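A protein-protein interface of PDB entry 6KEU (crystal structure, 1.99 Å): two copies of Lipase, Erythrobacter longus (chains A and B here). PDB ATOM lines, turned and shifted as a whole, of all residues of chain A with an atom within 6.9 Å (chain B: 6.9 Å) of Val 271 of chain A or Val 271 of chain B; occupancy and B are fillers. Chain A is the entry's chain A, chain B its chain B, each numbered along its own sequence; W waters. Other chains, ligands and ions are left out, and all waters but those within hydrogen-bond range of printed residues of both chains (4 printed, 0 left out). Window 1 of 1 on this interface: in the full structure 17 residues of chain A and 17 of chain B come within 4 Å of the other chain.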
ATOM      1  N   PRO A 241     -12.990   4.176   7.947  1.00  0.00           N
ATOM      2  CA  PRO A 241     -13.016   2.767   7.538  1.00  0.00           C
ATOM      3  C   PRO A 241     -14.447   2.257   7.479  1.00  0.00           C
ATOM      4  O   PRO A 241     -15.378   2.977   7.875  1.00  0.00           O
ATOM      5  CB  PRO A 241     -12.201   2.070   8.639  1.00  0.00           C
ATOM      6  CG  PRO A 241     -12.374   2.952   9.851  1.00  0.00           C
ATOM      7  CD  PRO A 241     -12.488   4.366   9.325  1.00  0.00           C
ATOM      8  N   PRO A 242     -14.673   1.051   6.951  1.00  0.00           N
ATOM      9  CA  PRO A 242     -16.027   0.481   6.985  1.00  0.00           C
ATOM     10  C   PRO A 242     -16.538   0.464   8.416  1.00  0.00           C
ATOM     11  O   PRO A 242     -15.781   0.190   9.349  1.00  0.00           O
ATOM     12  CB  PRO A 242     -15.834  -0.936   6.434  1.00  0.00           C
ATOM     13  CG  PRO A 242     -14.589  -0.861   5.609  1.00  0.00           C
ATOM     14  CD  PRO A 242     -13.704   0.118   6.347  1.00  0.00           C
ATOM     15  N   THR A 243     -17.819   0.797   8.594  1.00  0.00           N
ATOM     16  CA  THR A 243     -18.341   1.075   9.929  1.00  0.00           C
ATOM     17  C   THR A 243     -19.670   0.370  10.159  1.00  0.00           C
ATOM     18  O   THR A 243     -20.515   0.296   9.259  1.00  0.00           O
ATOM     19  CB  THR A 243     -18.523   2.595  10.145  1.00  0.00           C
ATOM     20  OG1 THR A 243     -17.257   3.253  10.006  1.00  0.00           O
ATOM     21  CG2 THR A 243     -19.070   2.896  11.554  1.00  0.00           C
ATOM     22  N   ILE A 244     -19.861  -0.128  11.378  1.00  0.00           N
ATOM     23  CA  ILE A 244     -21.180  -0.526  11.863  1.00  0.00           C
ATOM     24  C   ILE A 244     -21.508   0.347  13.065  1.00  0.00           C
ATOM     25  O   ILE A 244     -20.801   0.289  14.075  1.00  0.00           O
ATOM     26  CB  ILE A 244     -21.228  -2.010  12.245  1.00  0.00           C
ATOM     27  CG1 ILE A 244     -21.016  -2.879  11.011  1.00  0.00           C
ATOM     28  CG2 ILE A 244     -22.578  -2.343  12.922  1.00  0.00           C
ATOM     29  CD1 ILE A 244     -20.389  -4.204  11.344  1.00  0.00           C
ATOM     30  N   VAL A 245     -22.559   1.159  12.957  1.00  0.00           N
ATOM     31  CA  VAL A 245     -23.046   1.965  14.079  1.00  0.00           C
ATOM     32  C   VAL A 245     -24.297   1.299  14.637  1.00  0.00           C
ATOM     33  O   VAL A 245     -25.279   1.101  13.911  1.00  0.00           O
ATOM     34  CB  VAL A 245     -23.364   3.408  13.660  1.00  0.00           C
ATOM     35  CG1 VAL A 245     -23.948   4.180  14.866  1.00  0.00           C
ATOM     36  CG2 VAL A 245     -22.110   4.120  13.103  1.00  0.00           C
ATOM     37  N   TYR A 260     -23.549  10.536  13.789  1.00  0.00           N
ATOM     38  CA  TYR A 260     -22.299  10.011  13.252  1.00  0.00           C
ATOM     39  C   TYR A 260     -22.541   9.205  11.976  1.00  0.00           C
ATOM     40  O   TYR A 260     -21.827   9.373  10.979  1.00  0.00           O
ATOM     41  CB  TYR A 260     -21.562   9.175  14.308  1.00  0.00           C
ATOM     42  CG  TYR A 260     -20.211   8.696  13.806  1.00  0.00           C
ATOM     43  CD1 TYR A 260     -19.214   9.604  13.468  1.00  0.00           C
ATOM     44  CD2 TYR A 260     -19.949   7.342  13.630  1.00  0.00           C
ATOM     45  CE1 TYR A 260     -17.982   9.174  12.979  1.00  0.00           C
ATOM     46  CE2 TYR A 260     -18.723   6.904  13.149  1.00  0.00           C
ATOM     47  CZ  TYR A 260     -17.749   7.822  12.820  1.00  0.00           C
ATOM     48  OH  TYR A 260     -16.537   7.382  12.329  1.00  0.00           O
ATOM     49  N   ALA A 261     -23.548   8.327  11.977  1.00  0.00           N
ATOM     50  CA  ALA A 261     -23.816   7.545  10.773  1.00  0.00           C
ATOM     51  C   ALA A 261     -24.207   8.448   9.608  1.00  0.00           C
ATOM     52  O   ALA A 261     -23.784   8.217   8.467  1.00  0.00           O
ATOM     53  CB  ALA A 261     -24.909   6.498  11.035  1.00  0.00           C
ATOM     54  N   LYS A 262     -24.985   9.500   9.881  1.00  0.00           N
ATOM     55  CA  LYS A 262     -25.337  10.452   8.830  1.00  0.00           C
ATOM     56  C   LYS A 262     -24.098  11.128   8.258  1.00  0.00           C
ATOM     57  O   LYS A 262     -23.999  11.335   7.040  1.00  0.00           O
ATOM     58  CB  LYS A 262     -26.321  11.498   9.365  1.00  0.00           C
ATOM     59  CG  LYS A 262     -27.753  10.980   9.511  1.00  0.00           C
ATOM     60  CD  LYS A 262     -28.657  12.009  10.218  1.00  0.00           C
ATOM     61  CE  LYS A 262     -28.813  13.271   9.392  1.00  0.00           C
ATOM     62  NZ  LYS A 262     -29.644  14.306  10.077  1.00  0.00           N
ATOM     63  N   LEU A 264     -21.082   9.895   8.104  1.00  0.00           N
ATOM     64  CA  LEU A 264     -20.377   8.930   7.270  1.00  0.00           C
ATOM     65  C   LEU A 264     -21.034   8.803   5.898  1.00  0.00           C
ATOM     66  O   LEU A 264     -20.335   8.758   4.881  1.00  0.00           O
ATOM     67  CB  LEU A 264     -20.317   7.567   7.962  1.00  0.00           C
ATOM     68  CG  LEU A 264     -19.457   7.473   9.227  1.00  0.00           C
ATOM     69  CD1 LEU A 264     -19.437   6.055   9.767  1.00  0.00           C
ATOM     70  CD2 LEU A 264     -18.049   7.912   8.947  1.00  0.00           C
ATOM     71  N   VAL A 265     -22.369   8.739   5.843  1.00  0.00           N
ATOM     72  CA  VAL A 265     -23.042   8.713   4.543  1.00  0.00           C
ATOM     73  C   VAL A 265     -22.742   9.989   3.767  1.00  0.00           C
ATOM     74  O   VAL A 265     -22.488   9.956   2.557  1.00  0.00           O
ATOM     75  CB  VAL A 265     -24.559   8.519   4.707  1.00  0.00           C
ATOM     76  CG1 VAL A 265     -25.266   8.687   3.336  1.00  0.00           C
ATOM     77  CG2 VAL A 265     -24.871   7.158   5.328  1.00  0.00           C
ATOM     78  N   ARG A 269     -19.009   7.142   2.839  1.00  0.00           N
ATOM     79  CA  ARG A 269     -18.334   5.996   3.439  1.00  0.00           C
ATOM     80  C   ARG A 269     -19.336   4.864   3.631  1.00  0.00           C
ATOM     81  O   ARG A 269     -20.527   5.110   3.785  1.00  0.00           O
ATOM     82  CB  ARG A 269     -17.709   6.386   4.790  1.00  0.00           C
ATOM     83  CG  ARG A 269     -16.905   7.698   4.744  1.00  0.00           C
ATOM     84  CD  ARG A 269     -15.860   7.677   3.619  1.00  0.00           C
ATOM     85  NE  ARG A 269     -14.884   6.614   3.824  1.00  0.00           N
ATOM     86  CZ  ARG A 269     -14.195   6.026   2.855  1.00  0.00           C
ATOM     87  NH1 ARG A 269     -14.363   6.394   1.586  1.00  0.00           N
ATOM     88  NH2 ARG A 269     -13.338   5.065   3.157  1.00  0.00           N
ATOM     89  N   ASP A 270     -18.854   3.620   3.624  1.00  0.00           N
ATOM     90  CA  ASP A 270     -19.753   2.479   3.802  1.00  0.00           C
ATOM     91  C   ASP A 270     -20.123   2.330   5.275  1.00  0.00           C
ATOM     92  O   ASP A 270     -19.243   2.271   6.138  1.00  0.00           O
ATOM     93  CB  ASP A 270     -19.106   1.185   3.324  1.00  0.00           C
ATOM     94  CG  ASP A 270     -18.794   1.191   1.830  1.00  0.00           C
ATOM     95  OD1 ASP A 270     -19.361   2.010   1.076  1.00  0.00           O
ATOM     96  OD2 ASP A 270     -17.969   0.357   1.429  1.00  0.00           O
ATOM     97  N   VAL A 271     -21.416   2.233   5.567  1.00  0.00           N
ATOM     98  CA  VAL A 271     -21.835   2.154   6.965  1.00  0.00           C
ATOM     99  C   VAL A 271     -23.118   1.344   7.061  1.00  0.00           C
ATOM    100  O   VAL A 271     -24.009   1.448   6.209  1.00  0.00           O
ATOM    101  CB  VAL A 271     -21.987   3.564   7.580  1.00  0.00           C
ATOM    102  CG1 VAL A 271     -22.885   4.429   6.716  1.00  0.00           C
ATOM    103  CG2 VAL A 271     -22.497   3.490   9.051  1.00  0.00           C
ATOM    104  N   VAL A 272     -23.173   0.489   8.082  1.00  0.00           N
ATOM    105  CA  VAL A 272     -24.392  -0.190   8.509  1.00  0.00           C
ATOM    106  C   VAL A 272     -24.910   0.542   9.735  1.00  0.00           C
ATOM    107  O   VAL A 272     -24.203   0.641  10.748  1.00  0.00           O
ATOM    108  CB  VAL A 272     -24.130  -1.663   8.849  1.00  0.00           C
ATOM    109  CG1 VAL A 272     -25.451  -2.328   9.335  1.00  0.00           C
ATOM    110  CG2 VAL A 272     -23.506  -2.403   7.667  1.00  0.00           C
ATOM    111  N   TYR A 273     -26.126   1.064   9.661  1.00  0.00           N
ATOM    112  CA  TYR A 273     -26.746   1.706  10.816  1.00  0.00           C
ATOM    113  C   TYR A 273     -27.864   0.806  11.328  1.00  0.00           C
ATOM    114  O   TYR A 273     -28.817   0.531  10.591  1.00  0.00           O
ATOM    115  CB  TYR A 273     -27.296   3.090  10.476  1.00  0.00           C
ATOM    116  CG  TYR A 273     -27.926   3.729  11.696  1.00  0.00           C
ATOM    117  CD1 TYR A 273     -27.133   4.231  12.729  1.00  0.00           C
ATOM    118  CD2 TYR A 273     -29.307   3.788  11.835  1.00  0.00           C
ATOM    119  CE1 TYR A 273     -27.713   4.798  13.872  1.00  0.00           C
ATOM    120  CE2 TYR A 273     -29.890   4.343  12.964  1.00  0.00           C
ATOM    121  CZ  TYR A 273     -29.088   4.846  13.977  1.00  0.00           C
ATOM    122  OH  TYR A 273     -29.680   5.391  15.097  1.00  0.00           O
ATOM    123  N   LEU A 274     -27.745   0.354  12.582  1.00  0.00           N
ATOM    124  CA  LEU A 274     -28.741  -0.494  13.241  1.00  0.00           C
ATOM    125  C   LEU A 274     -29.207   0.178  14.525  1.00  0.00           C
ATOM    126  O   LEU A 274     -28.397   0.437  15.424  1.00  0.00           O
ATOM    127  CB  LEU A 274     -28.165  -1.874  13.562  1.00  0.00           C
ATOM    128  CG  LEU A 274     -27.572  -2.699  12.413  1.00  0.00           C
ATOM    129  CD1 LEU A 274     -27.052  -4.042  12.911  1.00  0.00           C
ATOM    130  CD2 LEU A 274     -28.605  -2.909  11.320  1.00  0.00           C
ATOM    131  N   GLU A 275     -30.506   0.453  14.621  1.00  0.00           N
ATOM    132  CA  GLU A 275     -31.084   1.086  15.804  1.00  0.00           C
ATOM    133  C   GLU A 275     -32.017   0.059  16.431  1.00  0.00           C
ATOM    134  O   GLU A 275     -33.083  -0.242  15.876  1.00  0.00           O
ATOM    135  CB  GLU A 275     -31.811   2.382  15.444  1.00  0.00           C
ATOM    136  CG  GLU A 275     -32.439   3.112  16.652  1.00  0.00           C
ATOM    137  CD  GLU A 275     -32.871   4.531  16.318  1.00  0.00           C
ATOM    138  OE1 GLU A 275     -32.080   5.273  15.683  1.00  0.00           O
ATOM    139  OE2 GLU A 275     -33.995   4.917  16.693  1.00  0.00           O
ATOM    140  N   MET A 307     -19.590  -7.330   6.839  1.00  0.00           N
ATOM    141  CA  MET A 307     -18.703  -6.240   6.442  1.00  0.00           C
ATOM    142  C   MET A 307     -17.250  -6.681   6.344  1.00  0.00           C
ATOM    143  O   MET A 307     -16.474  -6.034   5.633  1.00  0.00           O
ATOM    144  CB  MET A 307     -18.837  -5.062   7.410  1.00  0.00           C
ATOM    145  CG  MET A 307     -20.200  -4.366   7.331  1.00  0.00           C
ATOM    146  SD  MET A 307     -20.523  -3.511   5.764  1.00  0.00           S
ATOM    147  CE  MET A 307     -19.648  -1.961   6.067  1.00  0.00           C
ATOM    148  N   PRO B 241     -39.036   0.248   5.791  1.00  0.00           N
ATOM    149  CA  PRO B 241     -38.523  -1.110   6.020  1.00  0.00           C
ATOM    150  C   PRO B 241     -37.005  -1.113   6.075  1.00  0.00           C
ATOM    151  O   PRO B 241     -36.371  -0.123   5.679  1.00  0.00           O
ATOM    152  CB  PRO B 241     -39.031  -1.878   4.791  1.00  0.00           C
ATOM    153  CG  PRO B 241     -39.056  -0.832   3.718  1.00  0.00           C
ATOM    154  CD  PRO B 241     -39.525   0.429   4.411  1.00  0.00           C
ATOM    155  N   PRO B 242     -36.384  -2.199   6.550  1.00  0.00           N
ATOM    156  CA  PRO B 242     -34.923  -2.325   6.436  1.00  0.00           C
ATOM    157  C   PRO B 242     -34.497  -2.049   5.002  1.00  0.00           C
ATOM    158  O   PRO B 242     -35.176  -2.457   4.060  1.00  0.00           O
ATOM    159  CB  PRO B 242     -34.654  -3.782   6.830  1.00  0.00           C
ATOM    160  CG  PRO B 242     -35.850  -4.189   7.639  1.00  0.00           C
ATOM    161  CD  PRO B 242     -37.008  -3.439   7.047  1.00  0.00           C
ATOM    162  N   THR B 243     -33.379  -1.329   4.842  1.00  0.00           N
ATOM    163  CA  THR B 243     -32.988  -0.793   3.540  1.00  0.00           C
ATOM    164  C   THR B 243     -31.508  -1.026   3.258  1.00  0.00           C
ATOM    165  O   THR B 243     -30.663  -0.895   4.150  1.00  0.00           O
ATOM    166  CB  THR B 243     -33.274   0.717   3.464  1.00  0.00           C
ATOM    167  OG1 THR B 243     -34.675   0.949   3.666  1.00  0.00           O
ATOM    168  CG2 THR B 243     -32.860   1.284   2.103  1.00  0.00           C
ATOM    169  N   ILE B 244     -31.198  -1.378   2.011  1.00  0.00           N
ATOM    170  CA  ILE B 244     -29.836  -1.329   1.489  1.00  0.00           C
ATOM    171  C   ILE B 244     -29.825  -0.296   0.370  1.00  0.00           C
ATOM    172  O   ILE B 244     -30.470  -0.494  -0.671  1.00  0.00           O
ATOM    173  CB  ILE B 244     -29.365  -2.692   0.973  1.00  0.00           C
ATOM    174  CG1 ILE B 244     -29.339  -3.718   2.106  1.00  0.00           C
ATOM    175  CG2 ILE B 244     -27.990  -2.572   0.302  1.00  0.00           C
ATOM    176  CD1 ILE B 244     -29.305  -5.117   1.593  1.00  0.00           C
ATOM    177  N   VAL B 245     -29.114   0.808   0.575  1.00  0.00           N
ATOM    178  CA  VAL B 245     -28.914   1.813  -0.463  1.00  0.00           C
ATOM    179  C   VAL B 245     -27.533   1.585  -1.052  1.00  0.00           C
ATOM    180  O   VAL B 245     -26.528   1.634  -0.329  1.00  0.00           O
ATOM    181  CB  VAL B 245     -29.032   3.244   0.087  1.00  0.00           C
ATOM    182  CG1 VAL B 245     -28.725   4.239  -1.018  1.00  0.00           C
ATOM    183  CG2 VAL B 245     -30.414   3.510   0.671  1.00  0.00           C
ATOM    184  N   TYR B 260     -31.010  10.038   0.731  1.00  0.00           N
ATOM    185  CA  TYR B 260     -32.040   9.111   1.193  1.00  0.00           C
ATOM    186  C   TYR B 260     -31.543   8.278   2.372  1.00  0.00           C
ATOM    187  O   TYR B 260     -32.258   8.111   3.366  1.00  0.00           O
ATOM    188  CB  TYR B 260     -32.517   8.208   0.046  1.00  0.00           C
ATOM    189  CG  TYR B 260     -33.641   7.309   0.489  1.00  0.00           C
ATOM    190  CD1 TYR B 260     -34.851   7.841   0.918  1.00  0.00           C
ATOM    191  CD2 TYR B 260     -33.481   5.931   0.529  1.00  0.00           C
ATOM    192  CE1 TYR B 260     -35.883   7.019   1.359  1.00  0.00           C
ATOM    193  CE2 TYR B 260     -34.513   5.102   0.965  1.00  0.00           C
ATOM    194  CZ  TYR B 260     -35.703   5.656   1.384  1.00  0.00           C
ATOM    195  OH  TYR B 260     -36.728   4.840   1.818  1.00  0.00           O
ATOM    196  N   ALA B 261     -30.317   7.748   2.286  1.00  0.00           N
ATOM    197  CA  ALA B 261     -29.777   6.969   3.399  1.00  0.00           C
ATOM    198  C   ALA B 261     -29.651   7.825   4.662  1.00  0.00           C
ATOM    199  O   ALA B 261     -29.974   7.366   5.767  1.00  0.00           O
ATOM    200  CB  ALA B 261     -28.425   6.361   3.023  1.00  0.00           C
ATOM    201  N   LYS B 262     -29.212   9.079   4.518  1.00  0.00           N
ATOM    202  CA  LYS B 262     -29.175   9.985   5.671  1.00  0.00           C
ATOM    203  C   LYS B 262     -30.564  10.202   6.259  1.00  0.00           C
ATOM    204  O   LYS B 262     -30.727  10.251   7.486  1.00  0.00           O
ATOM    205  CB  LYS B 262     -28.555  11.330   5.284  1.00  0.00           C
ATOM    206  CG  LYS B 262     -27.075  11.264   4.953  1.00  0.00           C
ATOM    207  CD  LYS B 262     -26.570  12.603   4.425  1.00  0.00           C
ATOM    208  CE  LYS B 262     -26.890  13.701   5.423  1.00  0.00           C
ATOM    209  NZ  LYS B 262     -26.420  15.025   4.951  1.00  0.00           N
ATOM    210  N   LEU B 264     -33.043   8.117   6.296  1.00  0.00           N
ATOM    211  CA  LEU B 264     -33.461   6.932   7.042  1.00  0.00           C
ATOM    212  C   LEU B 264     -32.795   6.874   8.416  1.00  0.00           C
ATOM    213  O   LEU B 264     -33.448   6.549   9.415  1.00  0.00           O
ATOM    214  CB  LEU B 264     -33.149   5.666   6.244  1.00  0.00           C
ATOM    215  CG  LEU B 264     -33.951   5.497   4.950  1.00  0.00           C
ATOM    216  CD1 LEU B 264     -33.520   4.228   4.249  1.00  0.00           C
ATOM    217  CD2 LEU B 264     -35.442   5.457   5.237  1.00  0.00           C
ATOM    218  N   VAL B 265     -31.488   7.160   8.478  1.00  0.00           N
ATOM    219  CA  VAL B 265     -30.798   7.232   9.769  1.00  0.00           C
ATOM    220  C   VAL B 265     -31.456   8.281  10.656  1.00  0.00           C
ATOM    221  O   VAL B 265     -31.701   8.054  11.847  1.00  0.00           O
ATOM    222  CB  VAL B 265     -29.300   7.532   9.574  1.00  0.00           C
ATOM    223  CG1 VAL B 265     -28.611   7.743  10.941  1.00  0.00           C
ATOM    224  CG2 VAL B 265     -28.605   6.414   8.806  1.00  0.00           C
ATOM    225  N   ARG B 269     -34.152   4.388  11.177  1.00  0.00           N
ATOM    226  CA  ARG B 269     -34.428   3.149  10.457  1.00  0.00           C
ATOM    227  C   ARG B 269     -33.128   2.412  10.156  1.00  0.00           C
ATOM    228  O   ARG B 269     -32.073   3.026  10.011  1.00  0.00           O
ATOM    229  CB  ARG B 269     -35.178   3.445   9.161  1.00  0.00           C
ATOM    230  CG  ARG B 269     -36.346   4.444   9.321  1.00  0.00           C
ATOM    231  CD  ARG B 269     -37.331   4.005  10.414  1.00  0.00           C
ATOM    232  NE  ARG B 269     -37.949   2.708  10.113  1.00  0.00           N
ATOM    233  CZ  ARG B 269     -38.399   1.874  11.044  1.00  0.00           C
ATOM    234  NH1 ARG B 269     -38.293   2.195  12.334  1.00  0.00           N
ATOM    235  NH2 ARG B 269     -38.948   0.715  10.700  1.00  0.00           N
ATOM    236  N   ASP B 270     -33.209   1.083  10.067  1.00  0.00           N
ATOM    237  CA  ASP B 270     -32.022   0.279   9.788  1.00  0.00           C
ATOM    238  C   ASP B 270     -31.634   0.412   8.318  1.00  0.00           C
ATOM    239  O   ASP B 270     -32.455   0.179   7.430  1.00  0.00           O
ATOM    240  CB  ASP B 270     -32.279  -1.192  10.104  1.00  0.00           C
ATOM    241  CG  ASP B 270     -32.560  -1.446  11.580  1.00  0.00           C
ATOM    242  OD1 ASP B 270     -32.255  -0.578  12.429  1.00  0.00           O
ATOM    243  OD2 ASP B 270     -33.075  -2.538  11.882  1.00  0.00           O
ATOM    244  N   VAL B 271     -30.381   0.764   8.049  1.00  0.00           N
ATOM    245  CA  VAL B 271     -29.975   0.953   6.662  1.00  0.00           C
ATOM    246  C   VAL B 271     -28.519   0.553   6.503  1.00  0.00           C
ATOM    247  O   VAL B 271     -27.674   0.837   7.362  1.00  0.00           O
ATOM    248  CB  VAL B 271     -30.237   2.407   6.194  1.00  0.00           C
ATOM    249  CG1 VAL B 271     -29.698   3.401   7.199  1.00  0.00           C
ATOM    250  CG2 VAL B 271     -29.647   2.664   4.789  1.00  0.00           C
ATOM    251  N   VAL B 272     -28.242  -0.145   5.405  1.00  0.00           N
ATOM    252  CA  VAL B 272     -26.889  -0.391   4.933  1.00  0.00           C
ATOM    253  C   VAL B 272     -26.637   0.585   3.792  1.00  0.00           C
ATOM    254  O   VAL B 272     -27.387   0.596   2.806  1.00  0.00           O
ATOM    255  CB  VAL B 272     -26.718  -1.841   4.457  1.00  0.00           C
ATOM    256  CG1 VAL B 272     -25.304  -2.070   3.918  1.00  0.00           C
ATOM    257  CG2 VAL B 272     -27.074  -2.834   5.574  1.00  0.00           C
ATOM    258  N   TYR B 273     -25.601   1.418   3.918  1.00  0.00           N
ATOM    259  CA  TYR B 273     -25.233   2.345   2.848  1.00  0.00           C
ATOM    260  C   TYR B 273     -23.915   1.881   2.226  1.00  0.00           C
ATOM    261  O   TYR B 273     -22.893   1.784   2.915  1.00  0.00           O
ATOM    262  CB  TYR B 273     -25.141   3.796   3.350  1.00  0.00           C
ATOM    263  CG  TYR B 273     -24.739   4.723   2.229  1.00  0.00           C
ATOM    264  CD1 TYR B 273     -25.651   5.060   1.229  1.00  0.00           C
ATOM    265  CD2 TYR B 273     -23.429   5.188   2.115  1.00  0.00           C
ATOM    266  CE1 TYR B 273     -25.281   5.866   0.165  1.00  0.00           C
ATOM    267  CE2 TYR B 273     -23.048   5.995   1.049  1.00  0.00           C
ATOM    268  CZ  TYR B 273     -23.980   6.329   0.075  1.00  0.00           C
ATOM    269  OH  TYR B 273     -23.606   7.114  -0.998  1.00  0.00           O
ATOM    270  N   LEU B 274     -23.943   1.550   0.936  1.00  0.00           N
ATOM    271  CA  LEU B 274     -22.746   1.113   0.223  1.00  0.00           C
ATOM    272  C   LEU B 274     -22.512   2.046  -0.958  1.00  0.00           C
ATOM    273  O   LEU B 274     -23.378   2.176  -1.829  1.00  0.00           O
ATOM    274  CB  LEU B 274     -22.867  -0.341  -0.262  1.00  0.00           C
ATOM    275  CG  LEU B 274     -23.102  -1.432   0.793  1.00  0.00           C
ATOM    276  CD1 LEU B 274     -23.356  -2.794   0.119  1.00  0.00           C
ATOM    277  CD2 LEU B 274     -21.939  -1.515   1.783  1.00  0.00           C
ATOM    278  N   GLU B 275     -21.343   2.680  -0.994  1.00  0.00           N
ATOM    279  CA  GLU B 275     -20.972   3.581  -2.085  1.00  0.00           C
ATOM    280  C   GLU B 275     -19.789   2.930  -2.797  1.00  0.00           C
ATOM    281  O   GLU B 275     -18.671   2.907  -2.270  1.00  0.00           O
ATOM    282  CB  GLU B 275     -20.647   4.988  -1.574  1.00  0.00           C
ATOM    283  CG  GLU B 275     -20.301   5.982  -2.695  1.00  0.00           C
ATOM    284  CD  GLU B 275     -20.343   7.442  -2.256  1.00  0.00           C
ATOM    285  OE1 GLU B 275     -21.334   7.864  -1.616  1.00  0.00           O
ATOM    286  OE2 GLU B 275     -19.380   8.173  -2.572  1.00  0.00           O
ATOM    287  N   MET B 307     -29.207  -8.834   5.853  1.00  0.00           N
ATOM    288  CA  MET B 307     -30.369  -8.101   6.344  1.00  0.00           C
ATOM    289  C   MET B 307     -31.633  -8.948   6.372  1.00  0.00           C
ATOM    290  O   MET B 307     -32.580  -8.590   7.082  1.00  0.00           O
ATOM    291  CB  MET B 307     -30.617  -6.847   5.511  1.00  0.00           C
ATOM    292  CG  MET B 307     -29.497  -5.807   5.624  1.00  0.00           C
ATOM    293  SD  MET B 307     -29.452  -5.037   7.263  1.00  0.00           S
ATOM    294  CE  MET B 307     -30.762  -3.833   7.069  1.00  0.00           C
HETATM  295  O   HOH W   1     -17.368   0.839  -1.135  1.00  0.00           O
HETATM  296  O   HOH W   2     -33.772  -2.524  14.382  1.00  0.00           O
HETATM  297  O   HOH W   3     -34.689   0.777  13.639  1.00  0.00           O
HETATM  298  O   HOH W   4     -17.412   4.032   0.051  1.00  0.00           O
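OD1 of Asp 270 of chain A lies within hydrogen-bond range of N of Glu 275 of chain B, at 2.9 Å. The backbone carbonyl oxygen (O) of Val 271 of chain A lies within hydrogen-bond range of the backbone NH (N) of Tyr 273 of chain B (2.8 Å). The backbone carbonyl oxygen of Val 271 of chain B lies within hydrogen-bond range of the backbone NH of Tyr 273 of chain A, at 2.8 Å. N of Glu 275 of chain A sits at hydrogen-bond distance from OD1 of Asp 270 of chain B, at 3.0 Å.
The backbone carbonyl oxygen of Asp 270 of chain A lies within hydrogen-bond range of the backbone NH of Thr 243 of chain A (3.2 Å). N of Leu 274 of chain A is in hydrogen-bond range of O of Val 245 of chain A (2.9 Å). The side-chain hydroxyl (OH) of Tyr 273 of chain A lies within hydrogen-bond range of the side-chain carboxylate (OE1) of Glu 275 of chain A. The backbone NH of Val 245 of chain B sits at hydrogen-bond distance from the backbone carbonyl oxygen of Val 272 of chain B. N of Leu 274 of chain B is in hydrogen-bond range of O of Val 245 of chain B (2.9 Å).
Among the printed residues, merely in contact across the chains: Ala 261 of chain A with Val 265 of chain B (3.9 Å), Lys 262 of chain A with Lys 262 of chain B (3.7 Å), Lys 262 of chain A with Val 265 of chain B (3.6 Å), Val 265 of chain A with Ala 261 of chain B (3.9 Å), Val 265 of chain A with Lys 262 of chain B (3.5 Å), Val 265 of chain A with Tyr 273 of chain B (3.9 Å), Arg 269 of chain A with Tyr 273 of chain B (3.3 Å), Asp 270 of chain A with Tyr 273 of chain B (3.3 Å), Asp 270 of chain A with Leu 274 of chain B (3.6 Å), Val 271 of chain A with Val 271 of chain B (3.9 Å), Val 271 of chain A with Val 272 of chain B (3.6 Å), Val 272 of chain A with Val 271 of chain B (3.6 Å), Tyr 273 of chain A with Val 265 of chain B (3.9 Å), Tyr 273 of chain A with Arg 269 of chain B (3.4 Å), Tyr 273 of chain A with Asp 270 of chain B (3.3 Å) and Leu 274 of chain A with Asp 270 of chain B (3.6 Å).
Val 271 of chain A touches just these residues of chain B: Val 271 (3.9 Å), Val 272 (3.6 Å) and Tyr 273 (2.8 Å). Val 271 of chain B touches just these residues of chain A: Val 271 (3.9 Å), Val 272 (3.6 Å) and Tyr 273 (2.8 Å). Of the printed residues of chain A, Val 265 of chain B touches Ala 261, Lys 262 and Tyr 273. Printed residues of chain B within 4 Å of Leu 274 of chain A: Asp 270. Printed residues of chain B within 4 Å of Glu 275 of chain A: Asp 270. The nearest residue of chain B that does not touch Val 271 of chain A is Leu 274 of chain B (5.3 Å). The nearest printed residue of chain B that does not touch Val 265 of chain A is Glu 275 of chain B (4.8 Å).
Hydrophobic or aromatic side chains of chain A that line the printed part of chain B: Ala 261, Val 265 and Tyr 273. Among the printed residues, 20 pairs touch across the chains.
Ala 261 of chain A touches Val 265 of chain B, and with the chains exchanged Val 265 of chain A touches Ala 261 of chain B. Lys 262 of chain A touches Val 265 of chain B, and with the chains exchanged Val 265 of chain A touches Lys 262 of chain B. Arg 269 of chain A touches Tyr 273 of chain B, and with the chains exchanged Tyr 273 of chain A touches Arg 269 of chain B. Positions printed for both chains: 241, 242, 243, 244, 245, 260, 261, 262, 264, 265, 269, 270, 271, 272, 273, 274, 275 and 307.
Water W2 lies within hydrogen-bond range of OD2 of Asp 270 of chain B (2.6 Å) and O of Glu 275 of chain A (2.8 Å). Water W1 bridges the side-chain carboxylate of Asp 270 of chain A and the backbone carbonyl oxygen of Glu 275 of chain B. Water W3 lies within hydrogen-bond range of the backbone carbonyl oxygen (O) of Glu 275 of chain A (2.9 Å) and the side-chain carboxylate (OD1) of Asp 270 of chain B (3.0 Å).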
